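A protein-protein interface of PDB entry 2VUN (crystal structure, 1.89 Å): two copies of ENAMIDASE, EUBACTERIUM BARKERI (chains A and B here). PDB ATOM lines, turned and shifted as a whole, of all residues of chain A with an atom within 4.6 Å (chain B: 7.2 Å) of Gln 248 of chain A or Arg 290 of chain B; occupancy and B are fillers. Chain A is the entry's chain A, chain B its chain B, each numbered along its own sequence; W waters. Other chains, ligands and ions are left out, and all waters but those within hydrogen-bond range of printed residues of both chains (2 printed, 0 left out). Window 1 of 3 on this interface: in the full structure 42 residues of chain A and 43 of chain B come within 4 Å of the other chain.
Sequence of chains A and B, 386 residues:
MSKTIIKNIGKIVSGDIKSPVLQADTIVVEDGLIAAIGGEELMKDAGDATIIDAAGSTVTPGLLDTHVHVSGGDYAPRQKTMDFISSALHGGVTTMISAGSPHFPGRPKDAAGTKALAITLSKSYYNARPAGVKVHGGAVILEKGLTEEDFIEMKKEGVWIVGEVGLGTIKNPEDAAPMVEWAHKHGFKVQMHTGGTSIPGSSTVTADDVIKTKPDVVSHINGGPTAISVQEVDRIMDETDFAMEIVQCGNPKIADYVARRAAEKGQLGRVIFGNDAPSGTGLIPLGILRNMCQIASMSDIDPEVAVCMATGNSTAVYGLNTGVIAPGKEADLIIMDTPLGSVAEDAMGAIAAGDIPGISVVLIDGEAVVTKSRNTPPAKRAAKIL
The guanidinium group (NH1) of Arg 290 of chain A is in hydrogen-bond range of the backbone carbonyl oxygen (O) of Gln 248 of chain B, 3.0 Å away.
The backbone nitrogen of Pro 285 of chain B lies close to the backbone carbonyl oxygen of Thr 281 of chain A, at 3.2 Å.
The guanidinium group of Arg 290 of chain A sits close to the guanidinium group of Arg 290 of chain B (3.2 Å).
The side-chain amide nitrogen of Gln 248 of chain A sits close to the guanidinium group of Arg 290 of chain B (2.9 Å).
The backbone NH (N) of Leu 286 of chain B lies within hydrogen-bond range of the backbone carbonyl oxygen (O) of Thr 281 of chain A (3.3 Å).
OE1 of Gln 248 of chain B lies close to OD1 of Asn 291 of chain B.
The backbone carbonyl oxygen (O) of Asn 275 of chain A sits at hydrogen-bond distance from the backbone NH (N) of Cys 249 of chain A, at 2.9 Å.
The backbone NH (N) of Gln 248 of chain A is in hydrogen-bond range of the backbone carbonyl oxygen (O) of Gly 274 of chain A (3.0 Å).
NE of Arg 290 of chain B lies close to NE2 of Gln 248 of chain B (2.6 Å).
OD1 of Asn 291 of chain A lies close to OE1 of Gln 248 of chain A, 3.0 Å away.
NE of Arg 290 of chain A sits close to NE2 of Gln 248 of chain A.
Cys 249 of chain A touches Arg 290 of chain B (CA to NH1, 3.7 Å).
O of Thr 281 of chain A touches CG2 of Ile 284 of chain B, at 3.4 Å.
Arg 290 of chain B touches Thr 281 of chain A (CD to CG2, 3.6 Å).
CG2 of Ile 284 of chain A touches O of Thr 281 of chain B, at 3.5 Å.
Ile 284 of chain A touches Ile 284 of chain B (CG1 to CG1, 3.8 Å).
CD of Arg 290 of chain A touches CG2 of Thr 281 of chain B, at 3.7 Å.
Of chain B, only Arg 290 (2.9 Å) comes within 4 Å of Gln 248 of chain A.
Of the printed residues of chain A, Arg 290 of chain B touches Gln 248, Cys 249, Thr 281 and Arg 290.
Printed residues of chain A within 4 Å of Ile 284 of chain B: Thr 281 and Ile 284.
Of the printed residues of chain B, Thr 281 of chain A touches Ile 284 (3.4 Å), Pro 285 (3.0 Å), Leu 286 (3.3 Å) and Arg 290 (3.6 Å).
Of the printed residues of chain A, Pro 285 of chain B touches Thr 281 (3.0 Å).
Gly 250 of chain A touches none of the printed residues of chain B.
Leu 289 of chain B touches none of the printed residues of chain A.
The nearest residue of chain B that does not touch Gln 248 of chain A is Gln 248 of chain B (4.7 Å).
The nearest residue of chain A that does not touch Arg 290 of chain B is Gly 250 of chain A (4.2 Å).
The nearest printed residue of chain A that does not touch Thr 281 of chain B is Gly 287 of chain A (5.0 Å).
Of the 22 printed residues of chain B, 6 touch a printed residue of chain A.
Of the 12 printed residues of chain A, 5 touch a printed residue of chain B.
Hydrophobic or aromatic side chains of chain A that line the printed part of chain B: Ile 284.
Gln 248 of chain A touches Arg 290 of chain B, and with the chains exchanged Arg 290 of chain A touches Gln 248 of chain B.
Thr 281 of chain A touches Ile 284 of chain B, and with the chains exchanged Ile 284 of chain A touches Thr 281 of chain B.
Ile 284 of chain A touches its own counterpart, Ile 284 of chain B.
Arg 290 of chain A touches its own counterpart, Arg 290 of chain B.
7 positions are printed for both chains.
Of the 11 pairs that touch across the chains among the printed residues, 8 have their exchanged pair printed and touching as well.
Water W1 lies within hydrogen-bond range of OG1 of Thr 281 of chain B (2.7 Å) and NH1 of Arg 290 of chain A (2.8 Å).
Water W2 bridges the side-chain hydroxyl of Thr 281 of chain A and the guanidinium group of Arg 290 of chain B.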
ATOM      1  N   ILE A 246      -8.195  11.041  33.789  1.00  0.00           N
ATOM      2  CA  ILE A 246      -8.598  12.243  33.083  1.00  0.00           C
ATOM      3  C   ILE A 246     -10.102  12.177  32.906  1.00  0.00           C
ATOM      4  O   ILE A 246     -10.623  11.210  32.349  1.00  0.00           O
ATOM      5  CB  ILE A 246      -7.895  12.361  31.733  1.00  0.00           C
ATOM      6  CG1 ILE A 246      -6.400  12.671  31.965  1.00  0.00           C
ATOM      7  CG2 ILE A 246      -8.581  13.426  30.848  1.00  0.00           C
ATOM      8  CD1 ILE A 246      -5.582  12.662  30.696  1.00  0.00           C
ATOM      9  N   VAL A 247     -10.789  13.206  33.381  1.00  0.00           N
ATOM     10  CA  VAL A 247     -12.253  13.234  33.275  1.00  0.00           C
ATOM     11  C   VAL A 247     -12.717  14.253  32.249  1.00  0.00           C
ATOM     12  O   VAL A 247     -12.052  15.272  31.997  1.00  0.00           O
ATOM     13  CB  VAL A 247     -12.961  13.490  34.635  1.00  0.00           C
ATOM     14  CG1 VAL A 247     -12.606  12.393  35.643  1.00  0.00           C
ATOM     15  CG2 VAL A 247     -12.629  14.890  35.182  1.00  0.00           C
ATOM     16  N   GLN A 248     -13.872  13.966  31.664  1.00  0.00           N
ATOM     17  CA  GLN A 248     -14.485  14.841  30.681  1.00  0.00           C
ATOM     18  C   GLN A 248     -14.905  16.177  31.297  1.00  0.00           C
ATOM     19  O   GLN A 248     -14.727  17.234  30.685  1.00  0.00           O
ATOM     20  CB  GLN A 248     -15.681  14.108  30.067  1.00  0.00           C
ATOM     21  CG  GLN A 248     -16.645  14.936  29.252  1.00  0.00           C
ATOM     22  CD  GLN A 248     -16.061  15.477  27.965  1.00  0.00           C
ATOM     23  OE1 GLN A 248     -14.970  15.084  27.516  1.00  0.00           O
ATOM     24  NE2 GLN A 248     -16.783  16.408  27.368  1.00  0.00           N
ATOM     25  N   CYS A 249     -15.475  16.130  32.501  1.00  0.00           N
ATOM     26  CA  CYS A 249     -15.918  17.341  33.182  1.00  0.00           C
ATOM     27  C   CYS A 249     -14.778  17.964  33.991  1.00  0.00           C
ATOM     28  O   CYS A 249     -14.891  18.186  35.197  1.00  0.00           O
ATOM     29  CB  CYS A 249     -17.138  17.058  34.059  1.00  0.00           C
ATOM     30  SG  CYS A 249     -18.524  16.403  33.101  1.00  0.00           S
ATOM     31  N   GLY A 250     -13.673  18.224  33.308  1.00  0.00           N
ATOM     32  CA  GLY A 250     -12.500  18.796  33.944  1.00  0.00           C
ATOM     33  C   GLY A 250     -11.765  19.747  33.027  1.00  0.00           C
ATOM     34  O   GLY A 250     -12.258  20.111  31.960  1.00  0.00           O
ATOM     35  N   GLY A 274     -12.683   8.890  32.756  1.00  0.00           N
ATOM     36  CA  GLY A 274     -14.025   8.946  33.333  1.00  0.00           C
ATOM     37  C   GLY A 274     -14.720  10.230  32.908  1.00  0.00           C
ATOM     38  O   GLY A 274     -14.108  11.087  32.266  1.00  0.00           O
ATOM     39  N   ASN A 275     -16.001  10.358  33.244  1.00  0.00           N
ATOM     40  CA  ASN A 275     -16.744  11.597  32.981  1.00  0.00           C
ATOM     41  C   ASN A 275     -16.702  12.599  34.119  1.00  0.00           C
ATOM     42  O   ASN A 275     -16.660  13.806  33.874  1.00  0.00           O
ATOM     43  CB  ASN A 275     -18.215  11.303  32.661  1.00  0.00           C
ATOM     44  CG  ASN A 275     -18.454  11.082  31.190  1.00  0.00           C
ATOM     45  OD1 ASN A 275     -18.972  10.042  30.786  1.00  0.00           O
ATOM     46  ND2 ASN A 275     -18.083  12.054  30.380  1.00  0.00           N
ATOM     47  N   THR A 281     -21.424  20.268  35.779  1.00  0.00           N
ATOM     48  CA  THR A 281     -21.159  20.430  34.344  1.00  0.00           C
ATOM     49  C   THR A 281     -22.293  19.931  33.444  1.00  0.00           C
ATOM     50  O   THR A 281     -22.659  20.596  32.456  1.00  0.00           O
ATOM     51  CB  THR A 281     -19.826  19.749  33.945  1.00  0.00           C
ATOM     52  OG1 THR A 281     -18.752  20.422  34.601  1.00  0.00           O
ATOM     53  CG2 THR A 281     -19.596  19.812  32.427  1.00  0.00           C
ATOM     54  N   ILE A 284     -23.033  13.678  30.039  1.00  0.00           N
ATOM     55  CA  ILE A 284     -22.467  13.613  28.701  1.00  0.00           C
ATOM     56  C   ILE A 284     -22.301  12.145  28.301  1.00  0.00           C
ATOM     57  O   ILE A 284     -21.240  11.564  28.499  1.00  0.00           O
ATOM     58  CB  ILE A 284     -21.109  14.386  28.628  1.00  0.00           C
ATOM     59  CG1 ILE A 284     -21.262  15.823  29.175  1.00  0.00           C
ATOM     60  CG2 ILE A 284     -20.597  14.440  27.190  1.00  0.00           C
ATOM     61  CD1 ILE A 284     -19.932  16.581  29.355  1.00  0.00           C
ATOM     62  N   GLY A 287     -19.300  11.215  26.538  1.00  0.00           N
ATOM     63  CA  GLY A 287     -18.147  11.770  27.257  1.00  0.00           C
ATOM     64  C   GLY A 287     -16.847  10.989  27.141  1.00  0.00           C
ATOM     65  O   GLY A 287     -15.771  11.582  27.009  1.00  0.00           O
ATOM     66  N   ARG A 290     -15.576  11.497  23.689  1.00  0.00           N
ATOM     67  CA  ARG A 290     -15.029  12.850  23.567  1.00  0.00           C
ATOM     68  C   ARG A 290     -13.636  12.951  24.174  1.00  0.00           C
ATOM     69  O   ARG A 290     -12.774  13.621  23.613  1.00  0.00           O
ATOM     70  CB  ARG A 290     -15.970  13.883  24.195  1.00  0.00           C
ATOM     71  CG  ARG A 290     -17.180  14.197  23.318  1.00  0.00           C
ATOM     72  CD  ARG A 290     -18.271  14.911  24.096  1.00  0.00           C
ATOM     73  NE  ARG A 290     -17.751  16.065  24.817  1.00  0.00           N
ATOM     74  CZ  ARG A 290     -17.729  17.314  24.353  1.00  0.00           C
ATOM     75  NH1 ARG A 290     -18.206  17.607  23.152  1.00  0.00           N
ATOM     76  NH2 ARG A 290     -17.210  18.280  25.103  1.00  0.00           N
ATOM     77  N   ASN A 291     -13.437  12.279  25.313  1.00  0.00           N
ATOM     78  CA  ASN A 291     -12.124  12.158  25.953  1.00  0.00           C
ATOM     79  C   ASN A 291     -11.097  11.581  24.988  1.00  0.00           C
ATOM     80  O   ASN A 291      -9.994  12.103  24.854  1.00  0.00           O
ATOM     81  CB  ASN A 291     -12.209  11.234  27.168  1.00  0.00           C
ATOM     82  CG  ASN A 291     -12.675  11.938  28.425  1.00  0.00           C
ATOM     83  OD1 ASN A 291     -12.951  13.137  28.431  1.00  0.00           O
ATOM     84  ND2 ASN A 291     -12.746  11.186  29.513  1.00  0.00           N
ATOM     85  N   LEU B  63     -24.235  35.282  29.497  1.00  0.00           N
ATOM     86  CA  LEU B  63     -23.811  34.543  28.321  1.00  0.00           C
ATOM     87  C   LEU B  63     -24.980  34.201  27.406  1.00  0.00           C
ATOM     88  O   LEU B  63     -26.124  34.028  27.855  1.00  0.00           O
ATOM     89  CB  LEU B  63     -23.055  33.264  28.720  1.00  0.00           C
ATOM     90  CG  LEU B  63     -22.005  33.313  29.840  1.00  0.00           C
ATOM     91  CD1 LEU B  63     -21.436  31.917  30.096  1.00  0.00           C
ATOM     92  CD2 LEU B  63     -20.865  34.314  29.558  1.00  0.00           C
ATOM     93  N   GLN B 248     -20.092  23.505  21.680  1.00  0.00           N
ATOM     94  CA  GLN B 248     -19.495  22.640  22.689  1.00  0.00           C
ATOM     95  C   GLN B 248     -19.546  21.185  22.238  1.00  0.00           C
ATOM     96  O   GLN B 248     -18.576  20.442  22.418  1.00  0.00           O
ATOM     97  CB  GLN B 248     -20.206  22.856  24.030  1.00  0.00           C
ATOM     98  CG  GLN B 248     -19.976  21.803  25.109  1.00  0.00           C
ATOM     99  CD  GLN B 248     -18.577  21.799  25.705  1.00  0.00           C
ATOM    100  OE1 GLN B 248     -17.741  22.676  25.450  1.00  0.00           O
ATOM    101  NE2 GLN B 248     -18.313  20.785  26.505  1.00  0.00           N
ATOM    102  N   PHE B 273     -20.489  31.512  20.289  1.00  0.00           N
ATOM    103  CA  PHE B 273     -20.553  30.222  21.008  1.00  0.00           C
ATOM    104  C   PHE B 273     -21.970  29.685  21.177  1.00  0.00           C
ATOM    105  O   PHE B 273     -22.864  30.412  21.597  1.00  0.00           O
ATOM    106  CB  PHE B 273     -19.926  30.309  22.407  1.00  0.00           C
ATOM    107  CG  PHE B 273     -18.423  30.355  22.415  1.00  0.00           C
ATOM    108  CD1 PHE B 273     -17.678  29.603  21.518  1.00  0.00           C
ATOM    109  CD2 PHE B 273     -17.757  31.139  23.352  1.00  0.00           C
ATOM    110  CE1 PHE B 273     -16.283  29.647  21.535  1.00  0.00           C
ATOM    111  CE2 PHE B 273     -16.365  31.188  23.382  1.00  0.00           C
ATOM    112  CZ  PHE B 273     -15.630  30.443  22.472  1.00  0.00           C
ATOM    113  N   ASN B 275     -24.019  25.572  22.303  1.00  0.00           N
ATOM    114  CA  ASN B 275     -23.803  24.204  22.781  1.00  0.00           C
ATOM    115  C   ASN B 275     -24.047  23.130  21.731  1.00  0.00           C
ATOM    116  O   ASN B 275     -23.337  22.131  21.703  1.00  0.00           O
ATOM    117  CB  ASN B 275     -24.694  23.903  23.992  1.00  0.00           C
ATOM    118  CG  ASN B 275     -23.983  24.114  25.304  1.00  0.00           C
ATOM    119  OD1 ASN B 275     -24.369  24.966  26.106  1.00  0.00           O
ATOM    120  ND2 ASN B 275     -22.945  23.330  25.542  1.00  0.00           N
ATOM    121  N   THR B 281     -24.783  14.075  22.075  1.00  0.00           N
ATOM    122  CA  THR B 281     -23.651  14.265  22.989  1.00  0.00           C
ATOM    123  C   THR B 281     -24.082  14.350  24.448  1.00  0.00           C
ATOM    124  O   THR B 281     -23.436  13.777  25.330  1.00  0.00           O
ATOM    125  CB  THR B 281     -22.813  15.508  22.616  1.00  0.00           C
ATOM    126  OG1 THR B 281     -22.111  15.254  21.399  1.00  0.00           O
ATOM    127  CG2 THR B 281     -21.785  15.850  23.729  1.00  0.00           C
ATOM    128  N   ILE B 284     -25.279  20.034  28.629  1.00  0.00           N
ATOM    129  CA  ILE B 284     -24.120  20.561  29.338  1.00  0.00           C
ATOM    130  C   ILE B 284     -24.405  21.997  29.765  1.00  0.00           C
ATOM    131  O   ILE B 284     -24.108  22.932  29.017  1.00  0.00           O
ATOM    132  CB  ILE B 284     -22.842  20.473  28.438  1.00  0.00           C
ATOM    133  CG1 ILE B 284     -22.706  19.066  27.841  1.00  0.00           C
ATOM    134  CG2 ILE B 284     -21.576  20.876  29.233  1.00  0.00           C
ATOM    135  CD1 ILE B 284     -21.660  18.933  26.704  1.00  0.00           C
ATOM    136  N   PRO B 285     -25.032  22.182  30.949  1.00  0.00           N
ATOM    137  CA  PRO B 285     -25.335  23.541  31.412  1.00  0.00           C
ATOM    138  C   PRO B 285     -24.099  24.447  31.569  1.00  0.00           C
ATOM    139  O   PRO B 285     -24.223  25.667  31.455  1.00  0.00           O
ATOM    140  CB  PRO B 285     -26.032  23.318  32.760  1.00  0.00           C
ATOM    141  CG  PRO B 285     -25.663  21.895  33.169  1.00  0.00           C
ATOM    142  CD  PRO B 285     -25.547  21.155  31.877  1.00  0.00           C
ATOM    143  N   LEU B 286     -22.924  23.863  31.797  1.00  0.00           N
ATOM    144  CA  LEU B 286     -21.690  24.662  31.824  1.00  0.00           C
ATOM    145  C   LEU B 286     -20.992  24.731  30.460  1.00  0.00           C
ATOM    146  O   LEU B 286     -19.811  25.098  30.375  1.00  0.00           O
ATOM    147  CB  LEU B 286     -20.729  24.146  32.903  1.00  0.00           C
ATOM    148  CG  LEU B 286     -21.276  24.124  34.336  1.00  0.00           C
ATOM    149  CD1 LEU B 286     -20.147  23.799  35.317  1.00  0.00           C
ATOM    150  CD2 LEU B 286     -21.963  25.444  34.720  1.00  0.00           C
ATOM    151  N   GLY B 287     -21.731  24.401  29.402  1.00  0.00           N
ATOM    152  CA  GLY B 287     -21.179  24.312  28.047  1.00  0.00           C
ATOM    153  C   GLY B 287     -20.550  25.585  27.502  1.00  0.00           C
ATOM    154  O   GLY B 287     -19.468  25.545  26.887  1.00  0.00           O
ATOM    155  N   ILE B 288     -21.221  26.715  27.689  1.00  0.00           N
ATOM    156  CA  ILE B 288     -20.678  27.981  27.167  1.00  0.00           C
ATOM    157  C   ILE B 288     -19.409  28.386  27.921  1.00  0.00           C
ATOM    158  O   ILE B 288     -18.417  28.791  27.306  1.00  0.00           O
ATOM    159  CB  ILE B 288     -21.723  29.119  27.139  1.00  0.00           C
ATOM    160  CG1 ILE B 288     -22.960  28.702  26.324  1.00  0.00           C
ATOM    161  CG2 ILE B 288     -21.102  30.397  26.567  1.00  0.00           C
ATOM    162  CD1 ILE B 288     -22.673  28.259  24.853  1.00  0.00           C
ATOM    163  N   LEU B 289     -19.431  28.246  29.247  1.00  0.00           N
ATOM    164  CA  LEU B 289     -18.219  28.438  30.049  1.00  0.00           C
ATOM    165  C   LEU B 289     -17.092  27.521  29.590  1.00  0.00           C
ATOM    166  O   LEU B 289     -15.955  27.965  29.467  1.00  0.00           O
ATOM    167  CB  LEU B 289     -18.492  28.236  31.539  1.00  0.00           C
ATOM    168  CG  LEU B 289     -19.296  29.330  32.240  1.00  0.00           C
ATOM    169  CD1 LEU B 289     -19.606  28.887  33.655  1.00  0.00           C
ATOM    170  CD2 LEU B 289     -18.534  30.676  32.247  1.00  0.00           C
ATOM    171  N   ARG B 290     -17.409  26.255  29.324  1.00  0.00           N
ATOM    172  CA  ARG B 290     -16.410  25.301  28.839  1.00  0.00           C
ATOM    173  C   ARG B 290     -15.823  25.725  27.492  1.00  0.00           C
ATOM    174  O   ARG B 290     -14.616  25.603  27.280  1.00  0.00           O
ATOM    175  CB  ARG B 290     -16.986  23.883  28.758  1.00  0.00           C
ATOM    176  CG  ARG B 290     -17.057  23.181  30.109  1.00  0.00           C
ATOM    177  CD  ARG B 290     -17.990  21.986  30.061  1.00  0.00           C
ATOM    178  NE  ARG B 290     -17.615  21.050  29.002  1.00  0.00           N
ATOM    179  CZ  ARG B 290     -16.824  19.992  29.162  1.00  0.00           C
ATOM    180  NH1 ARG B 290     -16.292  19.714  30.343  1.00  0.00           N
ATOM    181  NH2 ARG B 290     -16.558  19.206  28.131  1.00  0.00           N
ATOM    182  N   ASN B 291     -16.673  26.236  26.599  1.00  0.00           N
ATOM    183  CA  ASN B 291     -16.209  26.792  25.327  1.00  0.00           C
ATOM    184  C   ASN B 291     -15.163  27.884  25.556  1.00  0.00           C
ATOM    185  O   ASN B 291     -14.112  27.901  24.907  1.00  0.00           O
ATOM    186  CB  ASN B 291     -17.373  27.389  24.537  1.00  0.00           C
ATOM    187  CG  ASN B 291     -18.174  26.348  23.775  1.00  0.00           C
ATOM    188  OD1 ASN B 291     -17.820  25.161  23.727  1.00  0.00           O
ATOM    189  ND2 ASN B 291     -19.257  26.799  23.154  1.00  0.00           N
ATOM    190  N   MET B 292     -15.469  28.792  26.479  1.00  0.00           N
ATOM    191  CA  MET B 292     -14.584  29.915  26.791  1.00  0.00           C
ATOM    192  C   MET B 292     -13.251  29.416  27.333  1.00  0.00           C
ATOM    193  O   MET B 292     -12.180  29.852  26.883  1.00  0.00           O
ATOM    194  CB  MET B 292     -15.267  30.857  27.787  1.00  0.00           C
ATOM    195  CG  MET B 292     -16.448  31.626  27.183  1.00  0.00           C
ATOM    196  SD  MET B 292     -17.635  32.260  28.404  1.00  0.00           S
ATOM    197  CE  MET B 292     -16.583  33.293  29.395  1.00  0.00           C
ATOM    198  N   CYS B 293     -13.322  28.478  28.275  1.00  0.00           N
ATOM    199  CA  CYS B 293     -12.130  27.915  28.891  1.00  0.00           C
ATOM    200  C   CYS B 293     -11.283  27.162  27.880  1.00  0.00           C
ATOM    201  O   CYS B 293     -10.060  27.301  27.865  1.00  0.00           O
ATOM    202  CB  CYS B 293     -12.504  27.004  30.052  1.00  0.00           C
ATOM    203  SG  CYS B 293     -13.202  27.894  31.461  1.00  0.00           S
ATOM    204  N   GLN B 294     -11.949  26.383  27.031  1.00  0.00           N
ATOM    205  CA  GLN B 294     -11.282  25.591  26.004  1.00  0.00           C
ATOM    206  C   GLN B 294     -10.556  26.493  24.999  1.00  0.00           C
ATOM    207  O   GLN B 294      -9.386  26.272  24.689  1.00  0.00           O
ATOM    208  CB  GLN B 294     -12.308  24.687  25.312  1.00  0.00           C
ATOM    209  CG  GLN B 294     -11.842  23.969  24.049  1.00  0.00           C
ATOM    210  CD  GLN B 294     -12.993  23.235  23.365  1.00  0.00           C
ATOM    211  OE1 GLN B 294     -14.092  23.104  23.933  1.00  0.00           O
ATOM    212  NE2 GLN B 294     -12.758  22.763  22.141  1.00  0.00           N
ATOM    213  N   ILE B 295     -11.249  27.517  24.504  1.00  0.00           N
ATOM    214  CA  ILE B 295     -10.668  28.398  23.493  1.00  0.00           C
ATOM    215  C   ILE B 295      -9.537  29.242  24.105  1.00  0.00           C
ATOM    216  O   ILE B 295      -8.473  29.383  23.510  1.00  0.00           O
ATOM    217  CB  ILE B 295     -11.766  29.257  22.773  1.00  0.00           C
ATOM    218  CG1 ILE B 295     -12.777  28.351  22.037  1.00  0.00           C
ATOM    219  CG2 ILE B 295     -11.167  30.273  21.810  1.00  0.00           C
ATOM    220  CD1 ILE B 295     -12.194  27.441  20.937  1.00  0.00           C
ATOM    221  N   ALA B 296      -9.756  29.769  25.305  1.00  0.00           N
ATOM    222  CA  ALA B 296      -8.725  30.567  25.972  1.00  0.00           C
ATOM    223  C   ALA B 296      -7.493  29.744  26.349  1.00  0.00           C
ATOM    224  O   ALA B 296      -6.359  30.174  26.101  1.00  0.00           O
ATOM    225  CB  ALA B 296      -9.288  31.294  27.196  1.00  0.00           C
ATOM    226  N   SER B 297      -7.705  28.561  26.918  1.00  0.00           N
ATOM    227  CA  SER B 297      -6.595  27.770  27.451  1.00  0.00           C
ATOM    228  C   SER B 297      -5.854  26.917  26.421  1.00  0.00           C
ATOM    229  O   SER B 297      -4.691  26.556  26.646  1.00  0.00           O
ATOM    230  CB  SER B 297      -7.060  26.880  28.602  1.00  0.00           C
ATOM    231  OG  SER B 297      -7.873  25.835  28.117  1.00  0.00           O
ATOM    232  N   GLY B 354      -7.907  27.221  32.107  1.00  0.00           N
ATOM    233  CA  GLY B 354      -8.765  26.084  31.771  1.00  0.00           C
ATOM    234  C   GLY B 354      -9.781  25.724  32.841  1.00  0.00           C
ATOM    235  O   GLY B 354     -10.506  24.739  32.683  1.00  0.00           O
ATOM    236  N   ILE B 356     -13.155  26.308  34.962  1.00  0.00           N
ATOM    237  CA  ILE B 356     -14.466  26.966  34.993  1.00  0.00           C
ATOM    238  C   ILE B 356     -14.540  27.925  36.189  1.00  0.00           C
ATOM    239  O   ILE B 356     -14.272  27.526  37.323  1.00  0.00           O
ATOM    240  CB  ILE B 356     -15.630  25.929  35.089  1.00  0.00           C
ATOM    241  CG1 ILE B 356     -15.615  25.012  33.859  1.00  0.00           C
ATOM    242  CG2 ILE B 356     -16.983  26.647  35.246  1.00  0.00           C
ATOM    243  CD1 ILE B 356     -16.676  23.933  33.863  1.00  0.00           C
ATOM    244  N   PRO B 357     -14.875  29.202  35.935  1.00  0.00           N
ATOM    245  CA  PRO B 357     -15.007  30.169  37.032  1.00  0.00           C
ATOM    246  C   PRO B 357     -16.209  29.872  37.938  1.00  0.00           C
ATOM    247  O   PRO B 357     -17.153  29.212  37.509  1.00  0.00           O
ATOM    248  CB  PRO B 357     -15.197  31.512  36.311  1.00  0.00           C
ATOM    249  CG  PRO B 357     -15.640  31.169  34.914  1.00  0.00           C
ATOM    250  CD  PRO B 357     -15.121  29.795  34.606  1.00  0.00           C
HETATM  251  O   HOH W   1     -19.630  16.290  21.148  1.00  0.00           O
HETATM  252  O   HOH W   2     -16.448  20.639  33.014  1.00  0.00           O
